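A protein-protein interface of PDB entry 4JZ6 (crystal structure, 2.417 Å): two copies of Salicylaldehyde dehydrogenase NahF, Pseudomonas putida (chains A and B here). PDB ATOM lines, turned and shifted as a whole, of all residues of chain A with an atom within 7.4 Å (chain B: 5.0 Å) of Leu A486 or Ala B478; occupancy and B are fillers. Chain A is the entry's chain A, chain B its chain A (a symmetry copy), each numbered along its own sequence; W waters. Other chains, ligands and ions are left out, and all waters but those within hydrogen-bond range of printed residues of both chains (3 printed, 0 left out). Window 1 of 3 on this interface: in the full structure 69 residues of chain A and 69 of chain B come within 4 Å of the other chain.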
ATOM      1  N   GLN A 136     -20.384 -16.334   4.844  1.00  0.00           N
ATOM      2  CA  GLN A 136     -21.271 -16.890   3.834  1.00  0.00           C
ATOM      3  C   GLN A 136     -20.557 -17.623   2.704  1.00  0.00           C
ATOM      4  O   GLN A 136     -19.379 -17.394   2.431  1.00  0.00           O
ATOM      5  CB  GLN A 136     -22.158 -15.781   3.266  1.00  0.00           C
ATOM      6  CG  GLN A 136     -23.136 -15.216   4.285  1.00  0.00           C
ATOM      7  CD  GLN A 136     -23.949 -14.071   3.732  1.00  0.00           C
ATOM      8  OE1 GLN A 136     -24.401 -13.201   4.477  1.00  0.00           O
ATOM      9  NE2 GLN A 136     -24.142 -14.061   2.420  1.00  0.00           N
ATOM     10  N   GLY A 137     -21.297 -18.515   2.054  1.00  0.00           N
ATOM     11  CA  GLY A 137     -20.813 -19.197   0.873  1.00  0.00           C
ATOM     12  C   GLY A 137     -21.614 -18.718  -0.317  1.00  0.00           C
ATOM     13  O   GLY A 137     -22.236 -17.653  -0.264  1.00  0.00           O
ATOM     14  N   GLU A 138     -21.606 -19.501  -1.391  1.00  0.00           N
ATOM     15  CA  GLU A 138     -22.233 -19.069  -2.631  1.00  0.00           C
ATOM     16  C   GLU A 138     -23.140 -20.143  -3.213  1.00  0.00           C
ATOM     17  O   GLU A 138     -22.922 -21.331  -2.999  1.00  0.00           O
ATOM     18  CB  GLU A 138     -21.165 -18.685  -3.658  1.00  0.00           C
ATOM     19  CG  GLU A 138     -20.266 -17.522  -3.251  1.00  0.00           C
ATOM     20  CD  GLU A 138     -19.070 -17.955  -2.415  1.00  0.00           C
ATOM     21  OE1 GLU A 138     -18.699 -17.202  -1.492  1.00  0.00           O
ATOM     22  OE2 GLU A 138     -18.491 -19.034  -2.684  1.00  0.00           O
ATOM     23  N   MET A 150     -23.296 -25.343  -4.626  1.00  0.00           N
ATOM     24  CA  MET A 150     -23.091 -24.284  -3.656  1.00  0.00           C
ATOM     25  C   MET A 150     -21.811 -24.493  -2.867  1.00  0.00           C
ATOM     26  O   MET A 150     -21.247 -25.587  -2.862  1.00  0.00           O
ATOM     27  CB  MET A 150     -24.272 -24.227  -2.687  1.00  0.00           C
ATOM     28  CG  MET A 150     -24.328 -25.416  -1.731  1.00  0.00           C
ATOM     29  SD  MET A 150     -25.870 -25.530  -0.802  1.00  0.00           S
ATOM     30  CE  MET A 150     -27.025 -26.039  -2.079  1.00  0.00           C
ATOM     31  N   THR A 151     -21.356 -23.432  -2.206  1.00  0.00           N
ATOM     32  CA  THR A 151     -20.257 -23.535  -1.260  1.00  0.00           C
ATOM     33  C   THR A 151     -20.754 -23.228   0.136  1.00  0.00           C
ATOM     34  O   THR A 151     -21.632 -22.386   0.321  1.00  0.00           O
ATOM     35  CB  THR A 151     -19.138 -22.556  -1.572  1.00  0.00           C
ATOM     36  OG1 THR A 151     -19.662 -21.222  -1.572  1.00  0.00           O
ATOM     37  CG2 THR A 151     -18.534 -22.870  -2.923  1.00  0.00           C
ATOM     38  N   LEU A 152     -20.193 -23.921   1.119  1.00  0.00           N
ATOM     39  CA  LEU A 152     -20.523 -23.669   2.513  1.00  0.00           C
ATOM     40  C   LEU A 152     -19.261 -23.265   3.256  1.00  0.00           C
ATOM     41  O   LEU A 152     -18.172 -23.775   2.968  1.00  0.00           O
ATOM     42  CB  LEU A 152     -21.118 -24.919   3.164  1.00  0.00           C
ATOM     43  CG  LEU A 152     -22.377 -25.538   2.557  1.00  0.00           C
ATOM     44  CD1 LEU A 152     -22.853 -26.717   3.402  1.00  0.00           C
ATOM     45  CD2 LEU A 152     -23.467 -24.497   2.439  1.00  0.00           C
ATOM     46  N   ARG A 153     -19.399 -22.335   4.197  1.00  0.00           N
ATOM     47  CA  ARG A 153     -18.306 -22.034   5.113  1.00  0.00           C
ATOM     48  C   ARG A 153     -18.650 -22.518   6.513  1.00  0.00           C
ATOM     49  O   ARG A 153     -19.550 -21.990   7.164  1.00  0.00           O
ATOM     50  CB  ARG A 153     -17.958 -20.552   5.091  1.00  0.00           C
ATOM     51  CG  ARG A 153     -17.299 -20.132   3.789  1.00  0.00           C
ATOM     52  CD  ARG A 153     -16.583 -18.812   3.926  1.00  0.00           C
ATOM     53  NE  ARG A 153     -15.813 -18.496   2.729  1.00  0.00           N
ATOM     54  CZ  ARG A 153     -14.585 -18.948   2.494  1.00  0.00           C
ATOM     55  NH1 ARG A 153     -13.979 -19.747   3.372  1.00  0.00           N
ATOM     56  NH2 ARG A 153     -13.964 -18.601   1.373  1.00  0.00           N
ATOM     57  N   GLN A 154     -17.929 -23.545   6.955  1.00  0.00           N
ATOM     58  CA  GLN A 154     -18.222 -24.236   8.209  1.00  0.00           C
ATOM     59  C   GLN A 154     -17.055 -24.098   9.176  1.00  0.00           C
ATOM     60  O   GLN A 154     -15.977 -23.654   8.780  1.00  0.00           O
ATOM     61  CB  GLN A 154     -18.479 -25.714   7.927  1.00  0.00           C
ATOM     62  CG  GLN A 154     -19.661 -25.981   7.019  1.00  0.00           C
ATOM     63  CD  GLN A 154     -19.807 -27.458   6.715  1.00  0.00           C
ATOM     64  OE1 GLN A 154     -18.922 -28.062   6.104  1.00  0.00           O
ATOM     65  NE2 GLN A 154     -20.913 -28.058   7.164  1.00  0.00           N
ATOM     66  N   PRO A 155     -17.263 -24.464  10.452  1.00  0.00           N
ATOM     67  CA  PRO A 155     -16.143 -24.378  11.400  1.00  0.00           C
ATOM     68  C   PRO A 155     -15.054 -25.396  11.075  1.00  0.00           C
ATOM     69  O   PRO A 155     -15.333 -26.400  10.417  1.00  0.00           O
ATOM     70  CB  PRO A 155     -16.793 -24.722  12.745  1.00  0.00           C
ATOM     71  CG  PRO A 155     -18.242 -24.414  12.561  1.00  0.00           C
ATOM     72  CD  PRO A 155     -18.541 -24.751  11.133  1.00  0.00           C
ATOM     73  N   VAL A 156     -13.839 -25.145  11.551  1.00  0.00           N
ATOM     74  CA  VAL A 156     -12.703 -26.017  11.280  1.00  0.00           C
ATOM     75  C   VAL A 156     -12.487 -27.036  12.395  1.00  0.00           C
ATOM     76  O   VAL A 156     -12.384 -28.236  12.144  1.00  0.00           O
ATOM     77  CB  VAL A 156     -11.411 -25.187  11.099  1.00  0.00           C
ATOM     78  CG1 VAL A 156     -10.200 -26.093  10.985  1.00  0.00           C
ATOM     79  CG2 VAL A 156     -11.529 -24.279   9.882  1.00  0.00           C
ATOM     80  N   ARG A 240      -5.697 -26.160  12.668  1.00  0.00           N
ATOM     81  CA  ARG A 240      -4.930 -25.095  12.028  1.00  0.00           C
ATOM     82  C   ARG A 240      -4.168 -24.295  13.074  1.00  0.00           C
ATOM     83  O   ARG A 240      -4.460 -24.374  14.269  1.00  0.00           O
ATOM     84  CB  ARG A 240      -5.829 -24.175  11.193  1.00  0.00           C
ATOM     85  CG  ARG A 240      -6.416 -24.839   9.956  1.00  0.00           C
ATOM     86  CD  ARG A 240      -7.375 -23.925   9.197  1.00  0.00           C
ATOM     87  NE  ARG A 240      -8.057 -24.649   8.125  1.00  0.00           N
ATOM     88  CZ  ARG A 240      -8.921 -24.108   7.268  1.00  0.00           C
ATOM     89  NH1 ARG A 240      -9.228 -22.819   7.339  1.00  0.00           N
ATOM     90  NH2 ARG A 240      -9.485 -24.867   6.330  1.00  0.00           N
ATOM     91  N   ARG A 263      -2.361 -26.150   7.841  1.00  0.00           N
ATOM     92  CA  ARG A 263      -2.324 -24.779   7.358  1.00  0.00           C
ATOM     93  C   ARG A 263      -1.924 -23.813   8.465  1.00  0.00           C
ATOM     94  O   ARG A 263      -2.358 -23.946   9.615  1.00  0.00           O
ATOM     95  CB  ARG A 263      -3.683 -24.384   6.779  1.00  0.00           C
ATOM     96  CG  ARG A 263      -3.829 -22.907   6.436  1.00  0.00           C
ATOM     97  CD  ARG A 263      -5.113 -22.680   5.673  1.00  0.00           C
ATOM     98  NE  ARG A 263      -5.393 -21.272   5.413  1.00  0.00           N
ATOM     99  CZ  ARG A 263      -6.499 -20.854   4.808  1.00  0.00           C
ATOM    100  NH1 ARG A 263      -7.402 -21.743   4.406  1.00  0.00           N
ATOM    101  NH2 ARG A 263      -6.704 -19.560   4.596  1.00  0.00           N
ATOM    102  N   ASP A 481     -11.750 -16.904   5.803  1.00  0.00           N
ATOM    103  CA  ASP A 481     -11.233 -18.090   5.143  1.00  0.00           C
ATOM    104  C   ASP A 481     -10.182 -18.791   5.999  1.00  0.00           C
ATOM    105  O   ASP A 481      -9.946 -19.990   5.856  1.00  0.00           O
ATOM    106  CB  ASP A 481     -10.638 -17.722   3.788  1.00  0.00           C
ATOM    107  CG  ASP A 481     -10.058 -18.921   3.067  1.00  0.00           C
ATOM    108  OD1 ASP A 481     -10.832 -19.661   2.424  1.00  0.00           O
ATOM    109  OD2 ASP A 481      -8.826 -19.129   3.154  1.00  0.00           O
ATOM    110  N   THR A 484     -12.316 -21.134   8.498  1.00  0.00           N
ATOM    111  CA  THR A 484     -13.477 -21.855   8.003  1.00  0.00           C
ATOM    112  C   THR A 484     -13.073 -22.967   7.058  1.00  0.00           C
ATOM    113  O   THR A 484     -12.016 -22.909   6.420  1.00  0.00           O
ATOM    114  CB  THR A 484     -14.485 -20.931   7.273  1.00  0.00           C
ATOM    115  OG1 THR A 484     -13.844 -20.274   6.164  1.00  0.00           O
ATOM    116  CG2 THR A 484     -15.062 -19.895   8.237  1.00  0.00           C
ATOM    117  N   GLU A 485     -13.911 -23.995   6.995  1.00  0.00           N
ATOM    118  CA  GLU A 485     -13.814 -24.982   5.935  1.00  0.00           C
ATOM    119  C   GLU A 485     -14.681 -24.479   4.802  1.00  0.00           C
ATOM    120  O   GLU A 485     -15.833 -24.096   5.030  1.00  0.00           O
ATOM    121  CB  GLU A 485     -14.332 -26.351   6.390  1.00  0.00           C
ATOM    122  CG  GLU A 485     -13.526 -27.027   7.485  1.00  0.00           C
ATOM    123  CD  GLU A 485     -12.094 -27.333   7.066  1.00  0.00           C
ATOM    124  OE1 GLU A 485     -11.748 -27.137   5.875  1.00  0.00           O
ATOM    125  OE2 GLU A 485     -11.315 -27.775   7.941  1.00  0.00           O
ATOM    126  N   LEU A 486     -14.127 -24.452   3.595  1.00  0.00           N
ATOM    127  CA  LEU A 486     -14.916 -24.147   2.410  1.00  0.00           C
ATOM    128  C   LEU A 486     -15.284 -25.459   1.739  1.00  0.00           C
ATOM    129  O   LEU A 486     -14.417 -26.202   1.289  1.00  0.00           O
ATOM    130  CB  LEU A 486     -14.148 -23.244   1.440  1.00  0.00           C
ATOM    131  CG  LEU A 486     -14.884 -22.916   0.138  1.00  0.00           C
ATOM    132  CD1 LEU A 486     -16.097 -22.042   0.406  1.00  0.00           C
ATOM    133  CD2 LEU A 486     -13.948 -22.246  -0.853  1.00  0.00           C
ATOM    134  N   LYS A 487     -16.576 -25.748   1.690  1.00  0.00           N
ATOM    135  CA  LYS A 487     -17.044 -27.013   1.153  1.00  0.00           C
ATOM    136  C   LYS A 487     -17.890 -26.796  -0.098  1.00  0.00           C
ATOM    137  O   LYS A 487     -18.783 -25.951  -0.120  1.00  0.00           O
ATOM    138  CB  LYS A 487     -17.844 -27.767   2.213  1.00  0.00           C
ATOM    139  CG  LYS A 487     -18.471 -29.053   1.710  1.00  0.00           C
ATOM    140  CD  LYS A 487     -19.299 -29.710   2.798  1.00  0.00           C
ATOM    141  CE  LYS A 487     -18.421 -30.262   3.918  1.00  0.00           C
ATOM    142  NZ  LYS A 487     -19.234 -30.796   5.055  1.00  0.00           N
ATOM    143  N   TRP A 488     -17.588 -27.550  -1.146  1.00  0.00           N
ATOM    144  CA  TRP A 488     -18.390 -27.511  -2.353  1.00  0.00           C
ATOM    145  C   TRP A 488     -19.408 -28.627  -2.246  1.00  0.00           C
ATOM    146  O   TRP A 488     -19.038 -29.800  -2.189  1.00  0.00           O
ATOM    147  CB  TRP A 488     -17.522 -27.700  -3.596  1.00  0.00           C
ATOM    148  CG  TRP A 488     -18.315 -27.836  -4.865  1.00  0.00           C
ATOM    149  CD1 TRP A 488     -19.455 -27.155  -5.204  1.00  0.00           C
ATOM    150  CD2 TRP A 488     -18.038 -28.724  -5.957  1.00  0.00           C
ATOM    151  NE1 TRP A 488     -19.896 -27.560  -6.445  1.00  0.00           N
ATOM    152  CE2 TRP A 488     -19.048 -28.525  -6.925  1.00  0.00           C
ATOM    153  CE3 TRP A 488     -17.029 -29.659  -6.217  1.00  0.00           C
ATOM    154  CZ2 TRP A 488     -19.074 -29.226  -8.130  1.00  0.00           C
ATOM    155  CZ3 TRP A 488     -17.059 -30.355  -7.415  1.00  0.00           C
ATOM    156  CH2 TRP A 488     -18.072 -30.133  -8.355  1.00  0.00           C
ATOM    157  N   LEU A 489     -20.686 -28.256  -2.197  1.00  0.00           N
ATOM    158  CA  LEU A 489     -21.764 -29.228  -2.026  1.00  0.00           C
ATOM    159  C   LEU A 489     -22.752 -29.202  -3.191  1.00  0.00           C
ATOM    160  O   LEU A 489     -23.152 -28.134  -3.660  1.00  0.00           O
ATOM    161  CB  LEU A 489     -22.501 -28.989  -0.706  1.00  0.00           C
ATOM    162  CG  LEU A 489     -23.613 -29.977  -0.343  1.00  0.00           C
ATOM    163  CD1 LEU A 489     -23.528 -30.355   1.130  1.00  0.00           C
ATOM    164  CD2 LEU A 489     -24.975 -29.388  -0.662  1.00  0.00           C
ATOM    165  N   GLY B 446     -13.700 -31.613   1.271  1.00  0.00           N
ATOM    166  CA  GLY B 446     -13.714 -30.431   0.435  1.00  0.00           C
ATOM    167  C   GLY B 446     -14.872 -30.450  -0.543  1.00  0.00           C
ATOM    168  O   GLY B 446     -15.391 -29.398  -0.915  1.00  0.00           O
ATOM    169  N   PRO B 462     -14.986 -24.308  -6.200  1.00  0.00           N
ATOM    170  CA  PRO B 462     -13.668 -24.490  -5.588  1.00  0.00           C
ATOM    171  C   PRO B 462     -13.333 -25.968  -5.483  1.00  0.00           C
ATOM    172  O   PRO B 462     -14.204 -26.764  -5.116  1.00  0.00           O
ATOM    173  CB  PRO B 462     -13.846 -23.890  -4.188  1.00  0.00           C
ATOM    174  CG  PRO B 462     -15.295 -23.987  -3.918  1.00  0.00           C
ATOM    175  CD  PRO B 462     -15.954 -23.742  -5.248  1.00  0.00           C
ATOM    176  N   ARG B 473      -6.789 -23.932  -2.743  1.00  0.00           N
ATOM    177  CA  ARG B 473      -7.886 -24.279  -3.634  1.00  0.00           C
ATOM    178  C   ARG B 473      -7.684 -23.837  -5.091  1.00  0.00           C
ATOM    179  O   ARG B 473      -7.322 -22.691  -5.360  1.00  0.00           O
ATOM    180  CB  ARG B 473      -9.190 -23.695  -3.075  1.00  0.00           C
ATOM    181  CG  ARG B 473     -10.377 -24.640  -3.144  1.00  0.00           C
ATOM    182  CD  ARG B 473     -10.855 -25.068  -1.759  1.00  0.00           C
ATOM    183  NE  ARG B 473      -9.927 -25.981  -1.100  1.00  0.00           N
ATOM    184  CZ  ARG B 473     -10.202 -26.674   0.004  1.00  0.00           C
ATOM    185  NH1 ARG B 473      -9.285 -27.474   0.530  1.00  0.00           N
ATOM    186  NH2 ARG B 473     -11.391 -26.577   0.581  1.00  0.00           N
ATOM    187  N   ASP B 475      -9.788 -23.605  -8.929  1.00  0.00           N
ATOM    188  CA  ASP B 475     -11.159 -23.376  -9.422  1.00  0.00           C
ATOM    189  C   ASP B 475     -12.008 -22.458  -8.538  1.00  0.00           C
ATOM    190  O   ASP B 475     -11.629 -22.133  -7.410  1.00  0.00           O
ATOM    191  CB  ASP B 475     -11.887 -24.698  -9.663  1.00  0.00           C
ATOM    192  CG  ASP B 475     -11.177 -25.570 -10.659  1.00  0.00           C
ATOM    193  OD1 ASP B 475     -10.744 -25.033 -11.700  1.00  0.00           O
ATOM    194  OD2 ASP B 475     -11.041 -26.786 -10.397  1.00  0.00           O
ATOM    195  N   GLY B 476     -13.158 -22.038  -9.062  1.00  0.00           N
ATOM    196  CA  GLY B 476     -14.051 -21.153  -8.330  1.00  0.00           C
ATOM    197  C   GLY B 476     -13.445 -19.786  -8.067  1.00  0.00           C
ATOM    198  O   GLY B 476     -12.368 -19.466  -8.567  1.00  0.00           O
ATOM    199  N   ARG B 477     -14.130 -18.967  -7.283  1.00  0.00           N
ATOM    200  CA  ARG B 477     -13.586 -17.664  -6.944  1.00  0.00           C
ATOM    201  C   ARG B 477     -12.411 -17.805  -5.974  1.00  0.00           C
ATOM    202  O   ARG B 477     -11.536 -16.941  -5.917  1.00  0.00           O
ATOM    203  CB  ARG B 477     -14.663 -16.768  -6.343  1.00  0.00           C
ATOM    204  CG  ARG B 477     -15.822 -16.437  -7.272  1.00  0.00           C
ATOM    205  CD  ARG B 477     -16.866 -15.617  -6.511  1.00  0.00           C
ATOM    206  NE  ARG B 477     -17.986 -15.169  -7.337  1.00  0.00           N
ATOM    207  CZ  ARG B 477     -19.088 -14.608  -6.846  1.00  0.00           C
ATOM    208  NH1 ARG B 477     -19.214 -14.439  -5.533  1.00  0.00           N
ATOM    209  NH2 ARG B 477     -20.067 -14.223  -7.658  1.00  0.00           N
ATOM    210  N   ALA B 478     -12.384 -18.903  -5.224  1.00  0.00           N
ATOM    211  CA  ALA B 478     -11.367 -19.098  -4.188  1.00  0.00           C
ATOM    212  C   ALA B 478      -9.934 -19.159  -4.722  1.00  0.00           C
ATOM    213  O   ALA B 478      -8.978 -18.870  -4.004  1.00  0.00           O
ATOM    214  CB  ALA B 478     -11.672 -20.341  -3.378  1.00  0.00           C
ATOM    215  N   VAL B 479      -9.787 -19.545  -5.982  1.00  0.00           N
ATOM    216  CA  VAL B 479      -8.469 -19.716  -6.559  1.00  0.00           C
ATOM    217  C   VAL B 479      -7.761 -18.361  -6.704  1.00  0.00           C
ATOM    218  O   VAL B 479      -6.531 -18.293  -6.765  1.00  0.00           O
ATOM    219  CB  VAL B 479      -8.553 -20.454  -7.913  1.00  0.00           C
ATOM    220  CG1 VAL B 479      -9.187 -19.564  -8.969  1.00  0.00           C
ATOM    221  CG2 VAL B 479      -7.175 -20.921  -8.363  1.00  0.00           C
ATOM    222  N   ILE B 480      -8.538 -17.282  -6.739  1.00  0.00           N
ATOM    223  CA  ILE B 480      -7.977 -15.948  -6.955  1.00  0.00           C
ATOM    224  C   ILE B 480      -7.018 -15.529  -5.848  1.00  0.00           C
ATOM    225  O   ILE B 480      -5.937 -15.014  -6.114  1.00  0.00           O
ATOM    226  CB  ILE B 480      -9.082 -14.890  -7.094  1.00  0.00           C
ATOM    227  CG1 ILE B 480      -9.925 -15.178  -8.338  1.00  0.00           C
ATOM    228  CG2 ILE B 480      -8.483 -13.490  -7.176  1.00  0.00           C
ATOM    229  CD1 ILE B 480     -11.126 -14.272  -8.481  1.00  0.00           C
ATOM    230  N   ASP B 481      -7.414 -15.765  -4.606  1.00  0.00           N
ATOM    231  CA  ASP B 481      -6.573 -15.421  -3.473  1.00  0.00           C
ATOM    232  C   ASP B 481      -5.256 -16.188  -3.502  1.00  0.00           C
ATOM    233  O   ASP B 481      -4.257 -15.754  -2.929  1.00  0.00           O
ATOM    234  CB  ASP B 481      -7.308 -15.702  -2.167  1.00  0.00           C
ATOM    235  CG  ASP B 481      -6.466 -15.386  -0.950  1.00  0.00           C
ATOM    236  OD1 ASP B 481      -6.408 -14.200  -0.556  1.00  0.00           O
ATOM    237  OD2 ASP B 481      -5.849 -16.322  -0.392  1.00  0.00           O
ATOM    238  N   GLU B 482      -5.255 -17.332  -4.170  1.00  0.00           N
ATOM    239  CA  GLU B 482      -4.061 -18.163  -4.232  1.00  0.00           C
ATOM    240  C   GLU B 482      -2.959 -17.513  -5.053  1.00  0.00           C
ATOM    241  O   GLU B 482      -1.775 -17.740  -4.809  1.00  0.00           O
ATOM    242  CB  GLU B 482      -4.398 -19.526  -4.822  1.00  0.00           C
ATOM    243  CG  GLU B 482      -5.473 -20.247  -4.068  1.00  0.00           C
ATOM    244  CD  GLU B 482      -4.972 -20.790  -2.750  1.00  0.00           C
ATOM    245  OE1 GLU B 482      -3.744 -20.725  -2.513  1.00  0.00           O
ATOM    246  OE2 GLU B 482      -5.808 -21.287  -1.961  1.00  0.00           O
HETATM  247  O   HOH W   1     -10.408 -26.961   3.854  1.00  0.00           O
HETATM  248  O   HOH W   2     -13.673 -26.115  -1.565  1.00  0.00           O
HETATM  249  O   HOH W   3      -7.289 -17.759   1.399  1.00  0.00           O
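1 position is printed for both chains. Of the 8 pairs that touch across the chains among the printed residues, none has its exchanged pair printed and touching as well.
The backbone NH (N) of Glu A138 sits at hydrogen-bond distance from the side-chain hydroxyl (OG1) of Thr A151 (2.6 Å). N of Arg B473 lies within hydrogen-bond range of OE2 of Glu B482, at 2.9 Å. The side-chain amide oxygen (OE1) of Gln A154 sits at hydrogen-bond distance from the side-chain amino group (NZ) of Lys A487 (2.9 Å). The backbone carbonyl oxygen (O) of Lys A487 sits at hydrogen-bond distance from the backbone NH (N) of Leu A152, 2.8 Å away.
N of Trp A488 sits at hydrogen-bond distance from O of Gly B446. The backbone carbonyl oxygen (O) of Leu A486 is in hydrogen-bond range of the guanidinium group (NH2) of Arg B473 (3.1 Å).
NH1 of Arg B477 touches CG of Glu A138, 3.98 Å away. Thr A151 touches Pro B462 (CG2 to CG, 3.6 Å). CB of Pro B462 touches CD2 of Leu A486, at 3.7 Å. CD2 of Leu A486 touches CB of Ala B478, at 3.9 Å. Lys A487 touches Gly B446. O of Pro B462 touches CB of Trp A488, 3.8 Å away.
Printed residues of chain B that touch a printed residue of chain A: Gly B446, Pro B462, Arg B473, Arg B477 and Ala B478. Hydrophobic or aromatic side chains of chain B that line the printed part of chain A: Pro B462 and Ala B478. Of the 19 printed residues of chain A, 5 touch a printed residue of chain B. Printed residues of chain A that touch a printed residue of chain B: Glu A138, Thr A151, Leu A486, Lys A487 and Trp A488. Among the printed residues, 8 pairs touch across the chains. Among the printed residues, no Asp or Glu carboxylate lies within 4 Å of a Lys or Arg side-chain nitrogen of the other chain.
Printed residues of chain B within 4 Å of Leu A486: Pro B462, Arg B473 and Ala B478. Ala B478 touches just one residue of chain A: Leu A486 (3.9 Å). Printed residues of chain A within 4 Å of Arg B477: Glu A138 (3.98 Å). Printed residues of chain B within 4 Å of Lys A487: Gly B446. Printed residues of chain A within 4 Å of Gly B446: Lys A487 (3.6 Å) and Trp A488 (2.9 Å). Gly A137 touches none of the printed residues of chain B. Gln A136 touches none of the printed residues of chain B. The nearest printed residue of chain B that does not touch Leu A486 is Gly B446 (4.003 Å).
Water W1 lies within hydrogen-bond range of OE1 of Glu A485, NH2 of Arg A240 and NH2 of Arg B473. Water W3 bridges OD2 of Asp A481 (2.7 Å) and OD2 of Asp B481 (2.7 Å). Water W2 lies within hydrogen-bond range of the backbone carbonyl oxygen (O) of Leu A486 (3.0 Å) and the guanidinium group (NH2) of Arg B473 (3.2 Å).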
